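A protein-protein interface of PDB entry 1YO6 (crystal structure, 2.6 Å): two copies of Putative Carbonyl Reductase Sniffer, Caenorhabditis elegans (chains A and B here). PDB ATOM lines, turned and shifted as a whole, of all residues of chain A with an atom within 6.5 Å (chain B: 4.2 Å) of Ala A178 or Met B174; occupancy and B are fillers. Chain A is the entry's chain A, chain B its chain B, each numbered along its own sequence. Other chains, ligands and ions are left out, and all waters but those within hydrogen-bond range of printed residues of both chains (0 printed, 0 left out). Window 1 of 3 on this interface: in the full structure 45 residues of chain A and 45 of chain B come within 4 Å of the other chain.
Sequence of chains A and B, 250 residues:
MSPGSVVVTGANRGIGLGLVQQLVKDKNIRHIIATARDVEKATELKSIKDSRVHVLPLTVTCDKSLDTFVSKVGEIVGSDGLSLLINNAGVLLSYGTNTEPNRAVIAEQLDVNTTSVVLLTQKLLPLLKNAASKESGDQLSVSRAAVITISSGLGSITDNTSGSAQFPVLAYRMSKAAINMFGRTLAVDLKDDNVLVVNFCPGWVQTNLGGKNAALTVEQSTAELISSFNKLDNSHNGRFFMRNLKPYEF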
ATOM      1  N   LEU A 110      18.315  25.110   7.867  1.00  0.00           N
ATOM      2  CA  LEU A 110      17.290  24.745   8.848  1.00  0.00           C
ATOM      3  C   LEU A 110      17.585  25.340  10.226  1.00  0.00           C
ATOM      4  O   LEU A 110      16.691  25.834  10.906  1.00  0.00           O
ATOM      5  CB  LEU A 110      17.180  23.219   8.947  1.00  0.00           C
ATOM      6  CG  LEU A 110      16.672  22.511   7.681  1.00  0.00           C
ATOM      7  CD1 LEU A 110      16.903  21.024   7.776  1.00  0.00           C
ATOM      8  CD2 LEU A 110      15.195  22.801   7.495  1.00  0.00           C
ATOM      9  N   THR A 114      14.786  27.771  10.857  1.00  0.00           N
ATOM     10  CA  THR A 114      13.807  27.015  11.609  1.00  0.00           C
ATOM     11  C   THR A 114      14.083  26.927  13.094  1.00  0.00           C
ATOM     12  O   THR A 114      13.518  27.679  13.889  1.00  0.00           O
ATOM     13  CB  THR A 114      13.653  25.573  11.040  1.00  0.00           C
ATOM     14  OG1 THR A 114      13.369  25.632   9.632  1.00  0.00           O
ATOM     15  CG2 THR A 114      12.508  24.832  11.757  1.00  0.00           C
ATOM     16  N   THR A 115      14.956  26.007  13.470  1.00  0.00           N
ATOM     17  CA  THR A 115      15.245  25.817  14.880  1.00  0.00           C
ATOM     18  C   THR A 115      15.591  27.097  15.672  1.00  0.00           C
ATOM     19  O   THR A 115      15.115  27.255  16.786  1.00  0.00           O
ATOM     20  CB  THR A 115      16.306  24.683  15.057  1.00  0.00           C
ATOM     21  OG1 THR A 115      17.144  24.941  16.197  1.00  0.00           O
ATOM     22  CG2 THR A 115      17.116  24.524  13.811  1.00  0.00           C
ATOM     23  N   VAL A 118      12.424  28.959  16.403  1.00  0.00           N
ATOM     24  CA  VAL A 118      11.644  28.246  17.414  1.00  0.00           C
ATOM     25  C   VAL A 118      12.252  28.448  18.783  1.00  0.00           C
ATOM     26  O   VAL A 118      11.543  28.652  19.764  1.00  0.00           O
ATOM     27  CB  VAL A 118      11.604  26.734  17.145  1.00  0.00           C
ATOM     28  CG1 VAL A 118      11.033  25.994  18.353  1.00  0.00           C
ATOM     29  CG2 VAL A 118      10.772  26.455  15.898  1.00  0.00           C
ATOM     30  N   GLY A 155       7.404  28.726   0.747  1.00  0.00           N
ATOM     31  CA  GLY A 155       7.214  27.770   1.818  1.00  0.00           C
ATOM     32  C   GLY A 155       5.942  26.971   1.630  1.00  0.00           C
ATOM     33  O   GLY A 155       5.786  25.905   2.218  1.00  0.00           O
ATOM     34  N   ARG A 173      13.059  26.299   0.958  1.00  0.00           N
ATOM     35  CA  ARG A 173      11.641  25.953   0.934  1.00  0.00           C
ATOM     36  C   ARG A 173      11.269  25.073   2.124  1.00  0.00           C
ATOM     37  O   ARG A 173      10.211  25.241   2.727  1.00  0.00           O
ATOM     38  CB  ARG A 173      11.283  25.183  -0.328  1.00  0.00           C
ATOM     39  CG  ARG A 173      11.179  25.961  -1.599  1.00  0.00           C
ATOM     40  CD  ARG A 173      10.742  24.975  -2.650  1.00  0.00           C
ATOM     41  NE  ARG A 173      10.621  25.537  -3.990  1.00  0.00           N
ATOM     42  CZ  ARG A 173       9.600  26.262  -4.435  1.00  0.00           C
ATOM     43  NH1 ARG A 173       8.570  26.551  -3.652  1.00  0.00           N
ATOM     44  NH2 ARG A 173       9.595  26.661  -5.701  1.00  0.00           N
ATOM     45  N   MET A 174      12.132  24.120   2.449  1.00  0.00           N
ATOM     46  CA  MET A 174      11.853  23.227   3.566  1.00  0.00           C
ATOM     47  C   MET A 174      11.883  23.959   4.893  1.00  0.00           C
ATOM     48  O   MET A 174      11.020  23.747   5.743  1.00  0.00           O
ATOM     49  CB  MET A 174      12.848  22.066   3.599  1.00  0.00           C
ATOM     50  CG  MET A 174      12.818  21.212   2.368  1.00  0.00           C
ATOM     51  SD  MET A 174      13.623  19.638   2.641  1.00  0.00           S
ATOM     52  CE  MET A 174      15.336  20.140   2.906  1.00  0.00           C
ATOM     53  N   SER A 175      12.871  24.831   5.060  1.00  0.00           N
ATOM     54  CA  SER A 175      13.018  25.589   6.292  1.00  0.00           C
ATOM     55  C   SER A 175      11.809  26.468   6.550  1.00  0.00           C
ATOM     56  O   SER A 175      11.494  26.758   7.696  1.00  0.00           O
ATOM     57  CB  SER A 175      14.265  26.459   6.229  1.00  0.00           C
ATOM     58  OG  SER A 175      14.049  27.557   5.372  1.00  0.00           O
ATOM     59  N   LYS A 176      11.136  26.900   5.488  1.00  0.00           N
ATOM     60  CA  LYS A 176       9.954  27.752   5.639  1.00  0.00           C
ATOM     61  C   LYS A 176       8.684  26.920   5.761  1.00  0.00           C
ATOM     62  O   LYS A 176       7.684  27.359   6.342  1.00  0.00           O
ATOM     63  CB  LYS A 176       9.827  28.705   4.457  1.00  0.00           C
ATOM     64  CG  LYS A 176      10.942  29.713   4.394  1.00  0.00           C
ATOM     65  CD  LYS A 176      10.872  30.677   5.553  1.00  0.00           C
ATOM     66  CE  LYS A 176      12.008  31.686   5.492  1.00  0.00           C
ATOM     67  NZ  LYS A 176      11.720  32.826   6.384  1.00  0.00           N
ATOM     68  N   ALA A 177       8.716  25.724   5.194  1.00  0.00           N
ATOM     69  CA  ALA A 177       7.574  24.849   5.300  1.00  0.00           C
ATOM     70  C   ALA A 177       7.523  24.488   6.786  1.00  0.00           C
ATOM     71  O   ALA A 177       6.473  24.552   7.436  1.00  0.00           O
ATOM     72  CB  ALA A 177       7.789  23.603   4.457  1.00  0.00           C
ATOM     73  N   ALA A 178       8.686  24.134   7.323  1.00  0.00           N
ATOM     74  CA  ALA A 178       8.783  23.767   8.724  1.00  0.00           C
ATOM     75  C   ALA A 178       8.314  24.935   9.575  1.00  0.00           C
ATOM     76  O   ALA A 178       7.427  24.781  10.416  1.00  0.00           O
ATOM     77  CB  ALA A 178      10.222  23.391   9.076  1.00  0.00           C
ATOM     78  N   ILE A 179       8.888  26.113   9.338  1.00  0.00           N
ATOM     79  CA  ILE A 179       8.514  27.274  10.121  1.00  0.00           C
ATOM     80  C   ILE A 179       7.039  27.584   9.952  1.00  0.00           C
ATOM     81  O   ILE A 179       6.438  28.191  10.823  1.00  0.00           O
ATOM     82  CB  ILE A 179       9.412  28.512   9.787  1.00  0.00           C
ATOM     83  CG1 ILE A 179       9.569  29.370  11.040  1.00  0.00           C
ATOM     84  CG2 ILE A 179       8.809  29.344   8.673  1.00  0.00           C
ATOM     85  CD1 ILE A 179       9.867  28.550  12.304  1.00  0.00           C
ATOM     86  N   ASN A 180       6.440  27.167   8.841  1.00  0.00           N
ATOM     87  CA  ASN A 180       5.010  27.401   8.686  1.00  0.00           C
ATOM     88  C   ASN A 180       4.270  26.377   9.539  1.00  0.00           C
ATOM     89  O   ASN A 180       3.179  26.650  10.024  1.00  0.00           O
ATOM     90  CB  ASN A 180       4.560  27.294   7.228  1.00  0.00           C
ATOM     91  CG  ASN A 180       4.865  28.553   6.424  1.00  0.00           C
ATOM     92  OD1 ASN A 180       5.101  29.623   6.990  1.00  0.00           O
ATOM     93  ND2 ASN A 180       4.839  28.431   5.097  1.00  0.00           N
ATOM     94  N   MET A 181       4.872  25.202   9.731  1.00  0.00           N
ATOM     95  CA  MET A 181       4.269  24.157  10.563  1.00  0.00           C
ATOM     96  C   MET A 181       4.382  24.558  12.032  1.00  0.00           C
ATOM     97  O   MET A 181       3.485  24.279  12.832  1.00  0.00           O
ATOM     98  CB  MET A 181       4.962  22.803  10.340  1.00  0.00           C
ATOM     99  CG  MET A 181       4.584  21.718  11.351  1.00  0.00           C
ATOM    100  SD  MET A 181       2.795  21.413  11.473  1.00  0.00           S
ATOM    101  CE  MET A 181       2.602  19.974  10.376  1.00  0.00           C
ATOM    102  N   PHE A 182       5.487  25.210  12.385  1.00  0.00           N
ATOM    103  CA  PHE A 182       5.682  25.671  13.753  1.00  0.00           C
ATOM    104  C   PHE A 182       4.565  26.651  14.095  1.00  0.00           C
ATOM    105  O   PHE A 182       3.857  26.467  15.086  1.00  0.00           O
ATOM    106  CB  PHE A 182       7.037  26.372  13.919  1.00  0.00           C
ATOM    107  CG  PHE A 182       7.224  27.033  15.268  1.00  0.00           C
ATOM    108  CD1 PHE A 182       7.078  26.305  16.445  1.00  0.00           C
ATOM    109  CD2 PHE A 182       7.573  28.380  15.355  1.00  0.00           C
ATOM    110  CE1 PHE A 182       7.277  26.906  17.687  1.00  0.00           C
ATOM    111  CE2 PHE A 182       7.777  28.996  16.603  1.00  0.00           C
ATOM    112  CZ  PHE A 182       7.629  28.254  17.765  1.00  0.00           C
ATOM    113  N   GLY A 183       4.405  27.686  13.270  1.00  0.00           N
ATOM    114  CA  GLY A 183       3.362  28.665  13.525  1.00  0.00           C
ATOM    115  C   GLY A 183       1.992  28.042  13.756  1.00  0.00           C
ATOM    116  O   GLY A 183       1.252  28.448  14.658  1.00  0.00           O
ATOM    117  N   THR A 185       1.322  25.080  14.818  1.00  0.00           N
ATOM    118  CA  THR A 185       1.362  24.327  16.057  1.00  0.00           C
ATOM    119  C   THR A 185       1.413  25.246  17.262  1.00  0.00           C
ATOM    120  O   THR A 185       0.799  24.973  18.289  1.00  0.00           O
ATOM    121  CB  THR A 185       2.585  23.417  16.078  1.00  0.00           C
ATOM    122  OG1 THR A 185       2.609  22.642  14.873  1.00  0.00           O
ATOM    123  CG2 THR A 185       2.554  22.500  17.295  1.00  0.00           C
ATOM    124  N   ILE B 106      15.976  19.368  18.408  1.00  0.00           N
ATOM    125  CA  ILE B 106      15.337  19.822  17.181  1.00  0.00           C
ATOM    126  C   ILE B 106      16.261  19.501  16.008  1.00  0.00           C
ATOM    127  O   ILE B 106      15.822  19.020  14.960  1.00  0.00           O
ATOM    128  CB  ILE B 106      15.094  21.349  17.210  1.00  0.00           C
ATOM    129  CG1 ILE B 106      14.164  21.713  18.369  1.00  0.00           C
ATOM    130  CG2 ILE B 106      14.505  21.804  15.886  1.00  0.00           C
ATOM    131  CD1 ILE B 106      14.111  23.210  18.662  1.00  0.00           C
ATOM    132  N   LEU B 170       6.331  18.511  18.109  1.00  0.00           N
ATOM    133  CA  LEU B 170       6.659  19.727  17.342  1.00  0.00           C
ATOM    134  C   LEU B 170       7.815  19.554  16.342  1.00  0.00           C
ATOM    135  O   LEU B 170       7.659  19.804  15.149  1.00  0.00           O
ATOM    136  CB  LEU B 170       6.972  20.897  18.303  1.00  0.00           C
ATOM    137  CG  LEU B 170       7.658  22.167  17.762  1.00  0.00           C
ATOM    138  CD1 LEU B 170       6.824  22.811  16.673  1.00  0.00           C
ATOM    139  CD2 LEU B 170       7.874  23.147  18.891  1.00  0.00           C
ATOM    140  N   ALA B 171       8.977  19.132  16.827  1.00  0.00           N
ATOM    141  CA  ALA B 171      10.114  18.956  15.936  1.00  0.00           C
ATOM    142  C   ALA B 171       9.795  17.897  14.890  1.00  0.00           C
ATOM    143  O   ALA B 171      10.217  18.007  13.743  1.00  0.00           O
ATOM    144  CB  ALA B 171      11.363  18.568  16.726  1.00  0.00           C
ATOM    145  N   TYR B 172       9.042  16.877  15.292  1.00  0.00           N
ATOM    146  CA  TYR B 172       8.662  15.802  14.382  1.00  0.00           C
ATOM    147  C   TYR B 172       7.755  16.357  13.284  1.00  0.00           C
ATOM    148  O   TYR B 172       8.000  16.135  12.101  1.00  0.00           O
ATOM    149  CB  TYR B 172       7.932  14.694  15.143  1.00  0.00           C
ATOM    150  CG  TYR B 172       7.586  13.488  14.300  1.00  0.00           C
ATOM    151  CD1 TYR B 172       8.555  12.533  13.980  1.00  0.00           C
ATOM    152  CD2 TYR B 172       6.289  13.303  13.816  1.00  0.00           C
ATOM    153  CE1 TYR B 172       8.239  11.420  13.198  1.00  0.00           C
ATOM    154  CE2 TYR B 172       5.959  12.195  13.032  1.00  0.00           C
ATOM    155  CZ  TYR B 172       6.933  11.255  12.725  1.00  0.00           C
ATOM    156  OH  TYR B 172       6.601  10.147  11.955  1.00  0.00           O
ATOM    157  N   ARG B 173       6.708  17.073  13.688  1.00  0.00           N
ATOM    158  CA  ARG B 173       5.777  17.673  12.744  1.00  0.00           C
ATOM    159  C   ARG B 173       6.534  18.515  11.715  1.00  0.00           C
ATOM    160  O   ARG B 173       6.286  18.420  10.507  1.00  0.00           O
ATOM    161  CB  ARG B 173       4.768  18.552  13.473  1.00  0.00           C
ATOM    162  CG  ARG B 173       3.601  17.818  14.150  1.00  0.00           C
ATOM    163  CD  ARG B 173       2.732  18.835  14.950  1.00  0.00           C
ATOM    164  NE  ARG B 173       1.441  18.313  15.401  1.00  0.00           N
ATOM    165  CZ  ARG B 173       0.501  17.840  14.586  1.00  0.00           C
ATOM    166  NH1 ARG B 173       0.699  17.817  13.277  1.00  0.00           N
ATOM    167  NH2 ARG B 173      -0.641  17.384  15.073  1.00  0.00           N
ATOM    168  N   MET B 174       7.467  19.332  12.182  1.00  0.00           N
ATOM    169  CA  MET B 174       8.237  20.166  11.263  1.00  0.00           C
ATOM    170  C   MET B 174       9.091  19.320  10.321  1.00  0.00           C
ATOM    171  O   MET B 174       9.182  19.615   9.134  1.00  0.00           O
ATOM    172  CB  MET B 174       9.142  21.135  12.033  1.00  0.00           C
ATOM    173  CG  MET B 174       8.424  21.983  13.056  1.00  0.00           C
ATOM    174  SD  MET B 174       9.459  23.329  13.637  1.00  0.00           S
ATOM    175  CE  MET B 174      10.550  22.492  14.834  1.00  0.00           C
ATOM    176  N   SER B 175       9.721  18.278  10.849  1.00  0.00           N
ATOM    177  CA  SER B 175      10.553  17.419  10.024  1.00  0.00           C
ATOM    178  C   SER B 175       9.727  16.830   8.881  1.00  0.00           C
ATOM    179  O   SER B 175      10.175  16.796   7.730  1.00  0.00           O
ATOM    180  CB  SER B 175      11.178  16.280  10.860  1.00  0.00           C
ATOM    181  OG  SER B 175      10.239  15.259  11.193  1.00  0.00           O
ATOM    182  N   LYS B 176       8.515  16.383   9.201  1.00  0.00           N
ATOM    183  CA  LYS B 176       7.639  15.781   8.212  1.00  0.00           C
ATOM    184  C   LYS B 176       7.110  16.772   7.203  1.00  0.00           C
ATOM    185  O   LYS B 176       6.998  16.454   6.024  1.00  0.00           O
ATOM    186  CB  LYS B 176       6.481  15.041   8.899  1.00  0.00           C
ATOM    187  CG  LYS B 176       6.923  13.741   9.582  1.00  0.00           C
ATOM    188  CD  LYS B 176       7.714  12.877   8.601  1.00  0.00           C
ATOM    189  CE  LYS B 176       8.248  11.592   9.226  1.00  0.00           C
ATOM    190  NZ  LYS B 176       8.947  10.752   8.196  1.00  0.00           N
ATOM    191  N   ALA B 177       6.788  17.975   7.658  1.00  0.00           N
ATOM    192  CA  ALA B 177       6.297  19.014   6.754  1.00  0.00           C
ATOM    193  C   ALA B 177       7.356  19.275   5.680  1.00  0.00           C
ATOM    194  O   ALA B 177       7.066  19.351   4.487  1.00  0.00           O
ATOM    195  CB  ALA B 177       6.027  20.300   7.536  1.00  0.00           C
ATOM    196  N   ALA B 178       8.594  19.400   6.134  1.00  0.00           N
ATOM    197  CA  ALA B 178       9.723  19.671   5.266  1.00  0.00           C
ATOM    198  C   ALA B 178       9.944  18.587   4.225  1.00  0.00           C
ATOM    199  O   ALA B 178      10.202  18.878   3.059  1.00  0.00           O
ATOM    200  CB  ALA B 178      10.987  19.847   6.116  1.00  0.00           C
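SD of Met A174 sits close to O of Ala B178 (3.5 Å).
The backbone NH of Thr A115 sits at hydrogen-bond distance from the backbone carbonyl oxygen of Leu A110 (3.1 Å). OG1 of Thr A114 lies within hydrogen-bond range of O of Ser A175. O of Met A181 is in hydrogen-bond range of OG1 of Thr A185 (2.8 Å).
Among the printed residues, merely in contact across the chains: Thr A115 with Ile B106 (3.5 Å), Phe A182 with Leu B170 (3.5 Å), Met A181 with Arg B173 (3.8 Å), Thr A185 with Arg B173 (3.8 Å), Met A181 with Met B174 (3.8 Å), Ala A178 with Met B174 (3.9 Å), Thr A114 with Met B174 (3.9 Å), Phe A182 with Met B174 (3.9 Å) and Met A181 with Ala B177 (3.9 Å).
Ala A178 touches just one residue of chain B: Met B174 (3.9 Å). Of chain A, only Thr A114, Ala A178, Met A181 and Phe A182 come within 4 Å of Met B174. Of the printed residues of chain A, Ala B177 touches Met A181 (3.9 Å). Of the printed residues of chain A, Leu B170 touches Phe A182. Of the printed residues of chain A, Ile B106 touches Thr A115 (3.5 Å). Of the printed residues of chain A, Arg B173 touches Met A181 and Thr A185. Asn A180 touches none of the printed residues of chain B. The nearest printed residue of chain B that does not touch Ala A178 is Ala B177 (4.6 Å). The nearest residue of chain A that does not touch Met B174 is Val A118 (4.1 Å). The nearest printed residue of chain B that does not touch Met A181 is Leu B170 (5.2 Å).
Along chain A the printed residues that touch a printed residue of chain B span positions 114 to 185. Of the 10 printed residues of chain B, 6 touch a printed residue of chain A. Printed residues of chain B that touch a printed residue of chain A: Ile B106, Leu B170, Arg B173, Met B174, Ala B177 and Ala B178. Among the printed residues, no Asp or Glu carboxylate lies within 4 Å of a Lys or Arg side-chain nitrogen of the other chain.
Met A174 touches Ala B178, and with the chains exchanged Ala A178 touches Met B174. 6 positions are printed for both chains.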
